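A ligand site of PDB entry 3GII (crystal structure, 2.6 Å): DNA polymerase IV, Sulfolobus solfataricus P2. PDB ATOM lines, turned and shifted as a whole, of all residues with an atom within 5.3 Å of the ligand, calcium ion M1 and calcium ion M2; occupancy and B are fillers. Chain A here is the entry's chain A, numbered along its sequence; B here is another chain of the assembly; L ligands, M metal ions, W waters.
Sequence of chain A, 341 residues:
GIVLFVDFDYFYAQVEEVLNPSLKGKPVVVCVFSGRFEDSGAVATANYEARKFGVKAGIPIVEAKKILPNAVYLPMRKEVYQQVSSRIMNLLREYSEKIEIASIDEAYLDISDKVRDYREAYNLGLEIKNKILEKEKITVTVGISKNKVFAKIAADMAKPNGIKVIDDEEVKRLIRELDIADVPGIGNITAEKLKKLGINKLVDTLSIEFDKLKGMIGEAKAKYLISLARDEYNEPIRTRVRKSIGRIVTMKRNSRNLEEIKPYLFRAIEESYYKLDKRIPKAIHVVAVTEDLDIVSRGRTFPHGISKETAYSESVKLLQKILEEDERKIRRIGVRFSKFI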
ATOM      1  N   ASP A   7     -14.209   8.535  30.999  1.00  0.00           N
ATOM      2  CA  ASP A   7     -14.969   9.322  30.026  1.00  0.00           C
ATOM      3  C   ASP A   7     -14.436   9.012  28.650  1.00  0.00           C
ATOM      4  O   ASP A   7     -13.255   9.152  28.401  1.00  0.00           O
ATOM      5  CB  ASP A   7     -14.813  10.812  30.277  1.00  0.00           C
ATOM      6  CG  ASP A   7     -15.421  11.636  29.180  1.00  0.00           C
ATOM      7  OD1 ASP A   7     -16.638  11.927  29.231  1.00  0.00           O
ATOM      8  OD2 ASP A   7     -14.682  11.998  28.229  1.00  0.00           O
ATOM      9  N   PHE A   8     -15.323   8.630  27.742  1.00  0.00           N
ATOM     10  CA  PHE A   8     -14.869   8.117  26.451  1.00  0.00           C
ATOM     11  C   PHE A   8     -14.409   9.274  25.553  1.00  0.00           C
ATOM     12  O   PHE A   8     -14.985  10.356  25.602  1.00  0.00           O
ATOM     13  CB  PHE A   8     -15.973   7.290  25.781  1.00  0.00           C
ATOM     14  CG  PHE A   8     -16.621   6.265  26.696  1.00  0.00           C
ATOM     15  CD1 PHE A   8     -15.991   5.812  27.851  1.00  0.00           C
ATOM     16  CD2 PHE A   8     -17.847   5.713  26.361  1.00  0.00           C
ATOM     17  CE1 PHE A   8     -16.588   4.847  28.658  1.00  0.00           C
ATOM     18  CE2 PHE A   8     -18.455   4.757  27.202  1.00  0.00           C
ATOM     19  CZ  PHE A   8     -17.826   4.329  28.330  1.00  0.00           C
ATOM     20  N   ASP A   9     -13.373   9.047  24.757  1.00  0.00           N
ATOM     21  CA  ASP A   9     -12.778  10.105  23.938  1.00  0.00           C
ATOM     22  C   ASP A   9     -13.594  10.372  22.671  1.00  0.00           C
ATOM     23  O   ASP A   9     -14.016   9.448  21.985  1.00  0.00           O
ATOM     24  CB  ASP A   9     -11.342   9.753  23.560  1.00  0.00           C
ATOM     25  CG  ASP A   9     -10.389   9.713  24.760  1.00  0.00           C
ATOM     26  OD1 ASP A   9     -10.687  10.334  25.806  1.00  0.00           O
ATOM     27  OD2 ASP A   9      -9.316   9.083  24.630  1.00  0.00           O
ATOM     28  N   TYR A  10     -13.816  11.655  22.377  1.00  0.00           N
ATOM     29  CA  TYR A  10     -14.651  12.100  21.242  1.00  0.00           C
ATOM     30  C   TYR A  10     -15.644  11.018  20.745  1.00  0.00           C
ATOM     31  O   TYR A  10     -15.684  10.666  19.568  1.00  0.00           O
ATOM     32  CB  TYR A  10     -13.760  12.665  20.106  1.00  0.00           C
ATOM     33  CG  TYR A  10     -12.775  11.691  19.494  1.00  0.00           C
ATOM     34  CD1 TYR A  10     -12.995  11.170  18.231  1.00  0.00           C
ATOM     35  CD2 TYR A  10     -11.599  11.324  20.169  1.00  0.00           C
ATOM     36  CE1 TYR A  10     -12.097  10.279  17.646  1.00  0.00           C
ATOM     37  CE2 TYR A  10     -10.695  10.428  19.589  1.00  0.00           C
ATOM     38  CZ  TYR A  10     -10.960   9.902  18.331  1.00  0.00           C
ATOM     39  OH  TYR A  10     -10.106   9.023  17.716  1.00  0.00           O
ATOM     40  N   PHE A  11     -16.465  10.544  21.668  1.00  0.00           N
ATOM     41  CA  PHE A  11     -17.143   9.240  21.546  1.00  0.00           C
ATOM     42  C   PHE A  11     -17.869   8.937  20.232  1.00  0.00           C
ATOM     43  O   PHE A  11     -17.514   7.972  19.557  1.00  0.00           O
ATOM     44  CB  PHE A  11     -18.101   9.054  22.714  1.00  0.00           C
ATOM     45  CG  PHE A  11     -18.688   7.677  22.804  1.00  0.00           C
ATOM     46  CD1 PHE A  11     -17.885   6.554  22.686  1.00  0.00           C
ATOM     47  CD2 PHE A  11     -20.055   7.504  23.014  1.00  0.00           C
ATOM     48  CE1 PHE A  11     -18.437   5.278  22.770  1.00  0.00           C
ATOM     49  CE2 PHE A  11     -20.613   6.241  23.099  1.00  0.00           C
ATOM     50  CZ  PHE A  11     -19.810   5.125  22.988  1.00  0.00           C
ATOM     51  N   TYR A  12     -18.898   9.708  19.874  1.00  0.00           N
ATOM     52  CA  TYR A  12     -19.662   9.351  18.676  1.00  0.00           C
ATOM     53  C   TYR A  12     -18.734   9.341  17.454  1.00  0.00           C
ATOM     54  O   TYR A  12     -18.824   8.458  16.596  1.00  0.00           O
ATOM     55  CB  TYR A  12     -20.822  10.323  18.394  1.00  0.00           C
ATOM     56  CG  TYR A  12     -21.938  10.393  19.417  1.00  0.00           C
ATOM     57  CD1 TYR A  12     -21.935   9.622  20.567  1.00  0.00           C
ATOM     58  CD2 TYR A  12     -23.015  11.242  19.209  1.00  0.00           C
ATOM     59  CE1 TYR A  12     -22.962   9.699  21.482  1.00  0.00           C
ATOM     60  CE2 TYR A  12     -24.040  11.336  20.120  1.00  0.00           C
ATOM     61  CZ  TYR A  12     -24.007  10.564  21.257  1.00  0.00           C
ATOM     62  OH  TYR A  12     -25.031  10.658  22.168  1.00  0.00           O
ATOM     63  N   ALA A  13     -17.840  10.309  17.396  1.00  0.00           N
ATOM     64  CA  ALA A  13     -16.905  10.388  16.299  1.00  0.00           C
ATOM     65  C   ALA A  13     -15.936   9.198  16.328  1.00  0.00           C
ATOM     66  O   ALA A  13     -15.573   8.646  15.284  1.00  0.00           O
ATOM     67  CB  ALA A  13     -16.148  11.709  16.330  1.00  0.00           C
ATOM     68  N   VAL A  32     -26.504  16.241  13.810  1.00  0.00           N
ATOM     69  CA  VAL A  32     -27.929  16.045  13.954  1.00  0.00           C
ATOM     70  C   VAL A  32     -28.634  16.878  12.890  1.00  0.00           C
ATOM     71  O   VAL A  32     -28.790  18.095  13.033  1.00  0.00           O
ATOM     72  CB  VAL A  32     -28.436  16.460  15.336  1.00  0.00           C
ATOM     73  CG1 VAL A  32     -29.904  16.042  15.498  1.00  0.00           C
ATOM     74  CG2 VAL A  32     -27.548  15.877  16.444  1.00  0.00           C
ATOM     75  N   VAL A  43     -24.111  20.240  15.304  1.00  0.00           N
ATOM     76  CA  VAL A  43     -23.042  19.250  15.457  1.00  0.00           C
ATOM     77  C   VAL A  43     -23.196  18.568  16.818  1.00  0.00           C
ATOM     78  O   VAL A  43     -23.298  19.231  17.836  1.00  0.00           O
ATOM     79  CB  VAL A  43     -21.651  19.940  15.353  1.00  0.00           C
ATOM     80  CG1 VAL A  43     -20.552  19.012  15.749  1.00  0.00           C
ATOM     81  CG2 VAL A  43     -21.415  20.477  13.945  1.00  0.00           C
ATOM     82  N   ALA A  44     -23.221  17.244  16.844  1.00  0.00           N
ATOM     83  CA  ALA A  44     -23.235  16.543  18.124  1.00  0.00           C
ATOM     84  C   ALA A  44     -21.840  16.512  18.706  1.00  0.00           C
ATOM     85  O   ALA A  44     -21.639  16.821  19.873  1.00  0.00           O
ATOM     86  CB  ALA A  44     -23.778  15.145  17.988  1.00  0.00           C
ATOM     87  N   THR A  45     -20.877  16.122  17.877  1.00  0.00           N
ATOM     88  CA  THR A  45     -19.460  16.111  18.276  1.00  0.00           C
ATOM     89  C   THR A  45     -18.607  15.936  17.039  1.00  0.00           C
ATOM     90  O   THR A  45     -19.113  15.595  15.961  1.00  0.00           O
ATOM     91  CB  THR A  45     -19.136  14.972  19.283  1.00  0.00           C
ATOM     92  OG1 THR A  45     -17.803  15.137  19.756  1.00  0.00           O
ATOM     93  CG2 THR A  45     -19.248  13.579  18.650  1.00  0.00           C
ATOM     94  N   TYR A  48     -10.875  15.262  17.231  1.00  0.00           N
ATOM     95  CA  TYR A  48      -9.915  16.282  17.602  1.00  0.00           C
ATOM     96  C   TYR A  48      -9.338  17.036  16.406  1.00  0.00           C
ATOM     97  O   TYR A  48      -8.983  18.212  16.513  1.00  0.00           O
ATOM     98  CB  TYR A  48      -8.842  15.678  18.501  1.00  0.00           C
ATOM     99  CG  TYR A  48      -9.311  15.626  19.929  1.00  0.00           C
ATOM    100  CD1 TYR A  48     -10.065  14.563  20.398  1.00  0.00           C
ATOM    101  CD2 TYR A  48      -9.049  16.693  20.797  1.00  0.00           C
ATOM    102  CE1 TYR A  48     -10.538  14.524  21.709  1.00  0.00           C
ATOM    103  CE2 TYR A  48      -9.513  16.672  22.117  1.00  0.00           C
ATOM    104  CZ  TYR A  48     -10.259  15.585  22.555  1.00  0.00           C
ATOM    105  OH  TYR A  48     -10.714  15.553  23.858  1.00  0.00           O
ATOM    106  N   ARG A  51     -11.824  19.571  15.585  1.00  0.00           N
ATOM    107  CA  ARG A  51     -11.912  20.562  16.677  1.00  0.00           C
ATOM    108  C   ARG A  51     -10.860  21.646  16.659  1.00  0.00           C
ATOM    109  O   ARG A  51     -11.133  22.781  17.050  1.00  0.00           O
ATOM    110  CB  ARG A  51     -11.824  19.902  18.032  1.00  0.00           C
ATOM    111  CG  ARG A  51     -13.126  19.388  18.461  1.00  0.00           C
ATOM    112  CD  ARG A  51     -13.060  18.811  19.829  1.00  0.00           C
ATOM    113  NE  ARG A  51     -13.913  17.643  19.897  1.00  0.00           N
ATOM    114  CZ  ARG A  51     -14.089  16.941  20.999  1.00  0.00           C
ATOM    115  NH1 ARG A  51     -13.495  17.304  22.129  1.00  0.00           N
ATOM    116  NH2 ARG A  51     -14.859  15.870  20.963  1.00  0.00           N
ATOM    117  N   ALA A  57     -19.366  20.668  19.461  1.00  0.00           N
ATOM    118  CA  ALA A  57     -20.764  20.391  19.752  1.00  0.00           C
ATOM    119  C   ALA A  57     -21.571  21.671  19.819  1.00  0.00           C
ATOM    120  O   ALA A  57     -21.124  22.634  20.420  1.00  0.00           O
ATOM    121  CB  ALA A  57     -20.878  19.660  21.048  1.00  0.00           C
ATOM    122  N   GLY A  58     -22.733  21.701  19.168  1.00  0.00           N
ATOM    123  CA  GLY A  58     -23.669  22.818  19.305  1.00  0.00           C
ATOM    124  C   GLY A  58     -23.668  23.875  18.216  1.00  0.00           C
ATOM    125  O   GLY A  58     -24.619  24.635  18.105  1.00  0.00           O
ATOM    126  N   MET A  76     -25.792  11.294  12.850  1.00  0.00           N
ATOM    127  CA  MET A  76     -25.707  10.659  14.148  1.00  0.00           C
ATOM    128  C   MET A  76     -26.501   9.388  14.165  1.00  0.00           C
ATOM    129  O   MET A  76     -27.662   9.393  13.835  1.00  0.00           O
ATOM    130  CB  MET A  76     -26.268  11.587  15.228  1.00  0.00           C
ATOM    131  CG  MET A  76     -26.008  11.057  16.591  1.00  0.00           C
ATOM    132  SD  MET A  76     -26.863  11.992  17.820  1.00  0.00           S
ATOM    133  CE  MET A  76     -28.590  11.654  17.439  1.00  0.00           C
ATOM    134  N   SER A 103     -23.568   9.078  32.171  1.00  0.00           N
ATOM    135  CA  SER A 103     -24.068   9.543  30.873  1.00  0.00           C
ATOM    136  C   SER A 103     -23.768   8.465  29.833  1.00  0.00           C
ATOM    137  O   SER A 103     -23.324   7.364  30.186  1.00  0.00           O
ATOM    138  CB  SER A 103     -23.415  10.866  30.475  1.00  0.00           C
ATOM    139  OG  SER A 103     -22.182  10.666  29.784  1.00  0.00           O
ATOM    140  N   ILE A 104     -23.997   8.763  28.557  1.00  0.00           N
ATOM    141  CA  ILE A 104     -23.753   7.786  27.497  1.00  0.00           C
ATOM    142  C   ILE A 104     -22.263   7.404  27.371  1.00  0.00           C
ATOM    143  O   ILE A 104     -21.926   6.338  26.834  1.00  0.00           O
ATOM    144  CB  ILE A 104     -24.252   8.302  26.130  1.00  0.00           C
ATOM    145  CG1 ILE A 104     -24.386   7.144  25.141  1.00  0.00           C
ATOM    146  CG2 ILE A 104     -23.317   9.358  25.553  1.00  0.00           C
ATOM    147  CD1 ILE A 104     -25.107   7.539  23.870  1.00  0.00           C
ATOM    148  N   ASP A 105     -21.389   8.270  27.863  1.00  0.00           N
ATOM    149  CA  ASP A 105     -19.954   8.054  27.661  1.00  0.00           C
ATOM    150  C   ASP A 105     -19.095   8.187  28.909  1.00  0.00           C
ATOM    151  O   ASP A 105     -17.886   8.354  28.792  1.00  0.00           O
ATOM    152  CB  ASP A 105     -19.422   8.999  26.582  1.00  0.00           C
ATOM    153  CG  ASP A 105     -18.915  10.309  27.149  1.00  0.00           C
ATOM    154  OD1 ASP A 105     -19.534  10.846  28.104  1.00  0.00           O
ATOM    155  OD2 ASP A 105     -17.854  10.796  26.672  1.00  0.00           O
ATOM    156  N   GLU A 106     -19.709   8.139  30.097  1.00  0.00           N
ATOM    157  CA  GLU A 106     -18.949   8.205  31.327  1.00  0.00           C
ATOM    158  C   GLU A 106     -19.593   7.462  32.497  1.00  0.00           C
ATOM    159  O   GLU A 106     -20.790   7.220  32.518  1.00  0.00           O
ATOM    160  CB  GLU A 106     -18.642   9.662  31.705  1.00  0.00           C
ATOM    161  CG  GLU A 106     -19.836  10.491  32.147  1.00  0.00           C
ATOM    162  CD  GLU A 106     -19.539  11.983  32.121  1.00  0.00           C
ATOM    163  OE1 GLU A 106     -19.608  12.634  33.196  1.00  0.00           O
ATOM    164  OE2 GLU A 106     -19.222  12.506  31.036  1.00  0.00           O
ATOM    165  N   LYS A 159      -7.499  14.793  29.223  1.00  0.00           N
ATOM    166  CA  LYS A 159      -8.037  14.342  27.925  1.00  0.00           C
ATOM    167  C   LYS A 159      -7.303  14.994  26.752  1.00  0.00           C
ATOM    168  O   LYS A 159      -6.825  16.116  26.860  1.00  0.00           O
ATOM    169  CB  LYS A 159      -9.570  14.446  27.820  1.00  0.00           C
ATOM    170  CG  LYS A 159     -10.241  15.681  28.362  1.00  0.00           C
ATOM    171  CD  LYS A 159     -11.770  15.669  28.031  1.00  0.00           C
ATOM    172  CE  LYS A 159     -12.580  14.668  28.887  1.00  0.00           C
ATOM    173  NZ  LYS A 159     -14.073  14.841  28.709  1.00  0.00           N
ATOM    174  N   PRO A 160      -7.166  14.259  25.636  1.00  0.00           N
ATOM    175  CA  PRO A 160      -7.630  12.916  25.296  1.00  0.00           C
ATOM    176  C   PRO A 160      -6.656  11.780  25.633  1.00  0.00           C
ATOM    177  O   PRO A 160      -5.503  12.042  25.985  1.00  0.00           O
ATOM    178  CB  PRO A 160      -7.806  13.010  23.783  1.00  0.00           C
ATOM    179  CG  PRO A 160      -6.662  13.848  23.371  1.00  0.00           C
ATOM    180  CD  PRO A 160      -6.431  14.840  24.495  1.00  0.00           C
ATOM    181  P    DC B   5     -31.826  23.728  16.743  1.00  0.00           P
ATOM    182  OP1  DC B   5     -32.707  23.922  15.569  1.00  0.00           O
ATOM    183  OP2  DC B   5     -32.192  24.301  18.073  1.00  0.00           O
ATOM    184  O5'  DC B   5     -31.556  22.169  16.821  1.00  0.00           O
ATOM    185  C5'  DC B   5     -31.443  21.469  15.594  1.00  0.00           C
ATOM    186  C4'  DC B   5     -31.193  20.021  15.860  1.00  0.00           C
ATOM    187  O4'  DC B   5     -29.899  19.941  16.507  1.00  0.00           O
ATOM    188  C3'  DC B   5     -32.225  19.427  16.804  1.00  0.00           C
ATOM    189  O3'  DC B   5     -32.520  18.052  16.457  1.00  0.00           O
ATOM    190  C2'  DC B   5     -31.532  19.558  18.156  1.00  0.00           C
ATOM    191  C1'  DC B   5     -30.087  19.297  17.738  1.00  0.00           C
ATOM    192  N1   DC B   5     -29.091  19.803  18.691  1.00  0.00           N
ATOM    193  C2   DC B   5     -28.189  18.896  19.224  1.00  0.00           C
ATOM    194  O2   DC B   5     -28.251  17.702  18.860  1.00  0.00           O
ATOM    195  N3   DC B   5     -27.267  19.350  20.099  1.00  0.00           N
ATOM    196  C4   DC B   5     -27.232  20.624  20.463  1.00  0.00           C
ATOM    197  N4   DC B   5     -26.286  20.973  21.335  1.00  0.00           N
ATOM    198  C5   DC B   5     -28.151  21.578  19.940  1.00  0.00           C
ATOM    199  C6   DC B   5     -29.059  21.122  19.066  1.00  0.00           C
ATOM    200  P   8OG B   6     -33.846  17.328  16.979  1.00  0.00           P
ATOM    201  OP1 8OG B   6     -34.150  16.124  16.140  1.00  0.00           O
ATOM    202  OP2 8OG B   6     -34.892  18.399  17.194  1.00  0.00           O
ATOM    203  O5' 8OG B   6     -33.405  16.782  18.422  1.00  0.00           O
ATOM    204  C5' 8OG B   6     -32.676  15.576  18.612  1.00  0.00           C
ATOM    205  C4' 8OG B   6     -32.245  15.764  20.030  1.00  0.00           C
ATOM    206  O4' 8OG B   6     -31.254  16.772  20.328  1.00  0.00           O
ATOM    207  C3' 8OG B   6     -32.852  15.283  21.110  1.00  0.00           C
ATOM    208  O3' 8OG B   6     -33.240  14.132  21.106  1.00  0.00           O
ATOM    209  C2' 8OG B   6     -32.487  16.088  22.349  1.00  0.00           C
ATOM    210  C1' 8OG B   6     -31.483  17.014  21.737  1.00  0.00           C
ATOM    211  N9  8OG B   6     -30.918  18.129  22.235  1.00  0.00           N
ATOM    212  C8  8OG B   6     -31.435  19.327  22.072  1.00  0.00           C
ATOM    213  N7  8OG B   6     -30.687  20.299  22.580  1.00  0.00           N
ATOM    214  C5  8OG B   6     -29.604  19.663  23.029  1.00  0.00           C
ATOM    215  C6  8OG B   6     -28.369  20.100  23.663  1.00  0.00           C
ATOM    216  O6  8OG B   6     -28.220  21.318  23.885  1.00  0.00           O
ATOM    217  N1  8OG B   6     -27.468  19.181  23.988  1.00  0.00           N
ATOM    218  C2  8OG B   6     -27.669  17.872  23.746  1.00  0.00           C
ATOM    219  N2  8OG B   6     -26.710  16.993  24.103  1.00  0.00           N
ATOM    220  N3  8OG B   6     -28.769  17.392  23.145  1.00  0.00           N
ATOM    221  C4  8OG B   6     -29.725  18.220  22.771  1.00  0.00           C
ATOM    222  O8  8OG B   6     -32.599  19.511  21.564  1.00  0.00           O
HETATM  223  P1  LIG L   1     -14.317  14.210  24.600  1.00  0.00           P
HETATM  224  O1  LIG L   1     -14.667  14.528  26.059  1.00  0.00           O
HETATM  225  O2  LIG L   1     -12.865  13.902  24.248  1.00  0.00           O
HETATM  226  O3  LIG L   1     -13.945  15.669  24.523  1.00  0.00           O
HETATM  227  O4  LIG L   1     -15.321  14.607  23.397  1.00  0.00           O
HETATM  228  P2  LIG L   1     -16.783  14.018  23.626  1.00  0.00           P
HETATM  229  O5  LIG L   1     -16.758  12.609  24.186  1.00  0.00           O
HETATM  230  O6  LIG L   1     -17.437  14.037  22.276  1.00  0.00           O
HETATM  231  O7  LIG L   1     -17.414  15.081  24.648  1.00  0.00           O
HETATM  232  P3  LIG L   1     -18.437  14.641  25.808  1.00  0.00           P
HETATM  233  O8  LIG L   1     -18.880  15.869  26.509  1.00  0.00           O
HETATM  234  O9  LIG L   1     -17.805  13.710  26.802  1.00  0.00           O
HETATM  235  O10 LIG L   1     -19.749  13.998  25.188  1.00  0.00           O
HETATM  236  C1  LIG L   1     -19.832  12.619  24.921  1.00  0.00           C
HETATM  237  C2  LIG L   1     -20.754  12.447  23.728  1.00  0.00           C
HETATM  238  O11 LIG L   1     -21.995  13.060  24.065  1.00  0.00           O
HETATM  239  C3  LIG L   1     -20.303  13.104  22.428  1.00  0.00           C
HETATM  240  O12 LIG L   1     -19.416  12.291  21.627  1.00  0.00           O
HETATM  241  C4  LIG L   1     -21.636  13.363  21.750  1.00  0.00           C
HETATM  242  C5  LIG L   1     -22.601  13.586  22.905  1.00  0.00           C
HETATM  243  N1  LIG L   1     -22.802  15.030  23.053  1.00  0.00           N
HETATM  244  C6  LIG L   1     -22.138  15.940  23.847  1.00  0.00           C
HETATM  245  N2  LIG L   1     -22.564  17.171  23.679  1.00  0.00           N
HETATM  246  C7  LIG L   1     -23.575  17.070  22.717  1.00  0.00           C
HETATM  247  C8  LIG L   1     -24.434  18.024  22.120  1.00  0.00           C
HETATM  248  O13 LIG L   1     -24.532  19.251  22.269  1.00  0.00           O
HETATM  249  N3  LIG L   1     -25.309  17.438  21.211  1.00  0.00           N
HETATM  250  C9  LIG L   1     -25.377  16.108  20.876  1.00  0.00           C
HETATM  251  N4  LIG L   1     -26.273  15.761  19.960  1.00  0.00           N
HETATM  252  N5  LIG L   1     -24.566  15.197  21.441  1.00  0.00           N
HETATM  253  C10 LIG L   1     -23.715  15.742  22.335  1.00  0.00           C
HETATM  254 CA    CA M   1     -18.673  12.949  28.823  1.00  0.00          CA
HETATM  255 CA    CA M   2     -16.081  12.240  26.395  1.00  0.00          CA
HETATM  256  O   HOH W   1     -21.376  13.584  28.484  1.00  0.00           O
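N3 of DC 5 of chain B sits at hydrogen-bond distance from N3 of the ligand, at 3.0 Å.
An oxygen (O1) of the ligand lies close to the side-chain amino group (NZ) of Lys 159 (2.7 Å).
The side-chain hydroxyl (OH) of Tyr 48 is in hydrogen-bond range of an oxygen (O2) of the ligand.
An oxygen (O6) of the ligand is in hydrogen-bond range of the side-chain hydroxyl (OG1) of Thr 45, 2.8 Å away.
O3 of the ligand is in salt-bridge range of NH1 of Arg 51, 2.9 Å away.
The backbone NH (N) of Tyr 10 is in hydrogen-bond range of an oxygen (O2) of the ligand (3.1 Å).
The backbone NH (N) of Tyr 12 lies within hydrogen-bond range of an oxygen (O12) of the ligand (3.2 Å).
A nitrogen (N3) of the ligand sits close to N2 of 8OG 6 of chain B (3.2 Å).
An oxygen (O12) of the ligand sits at hydrogen-bond distance from the backbone NH (N) of Phe 11, 3.4 Å away.
OG of Ser 103 sits close to N of Asp 105 (3.2 Å).
The side-chain carboxylate of Asp 7 sits close to the side-chain amino group of Lys 159 (2.9 Å).
NH2 of Arg 51 sits at hydrogen-bond distance from OG1 of Thr 45.
CA of Asp 9 touches O2 of the ligand, 3.8 Å away.
CG2 of Val 32 touches N4 of the ligand, 3.7 Å away.
Ala 44 touches the ligand (CB to N4, 3.2 Å).
Ala 57 touches the ligand (CB to O13, 3.9 Å).
Hydrophobic or aromatic side chains within 4 Å of the ligand: Phe 11, Tyr 12, Val 32, Ala 44, Tyr 48 and Ala 57.
Within 4 Å of the ligand: Asp 7, Phe 8, Asp 9, Tyr 10, Phe 11, Tyr 12, Val 32, Ala 44, Thr 45, Tyr 48, Arg 51, Ala 57, Asp 105, Lys 159, DC 5 of chain B and 8OG 6 of chain B.
The nearest printed residue that does not touch the ligand is Ile 104 (4.2 Å).
Of the 24 residues printed, 3 come within 4 Å of calcium ion M1.
Within 4 Å of calcium ion M2: Asp 7, Phe 8 and Asp 105.
Calcium ion M1 is bound by the side-chain carboxylate of Asp 7 (2.3 Å), the side-chain carboxylate of Glu 106 (2.3 Å), an oxygen (O9) of the ligand (2.3 Å), the side-chain carboxylate of Asp 105 (2.4 Å) and water W1 (2.8 Å).
Calcium ion M2 is bound by O9 of the ligand.
The side-chain carboxylate (OD2) of Asp 105 is bound to calcium ion M2 (2.3 Å).
Calcium ion M2 is bound by O of Phe 8 (2.3 Å).
Calcium ion M2 is bound by OD2 of Asp 7 (2.3 Å).
An oxygen (O5) of the ligand binds calcium ion M2 (2.3 Å).
An oxygen (O1) of the ligand binds calcium ion M2, 2.7 Å away.
Calcium ion M2 has six donor atoms within binding distance.
Slightly farther from calcium ion M2 lies the side-chain carboxylate (OD1) of Asp 7 (2.9 Å).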
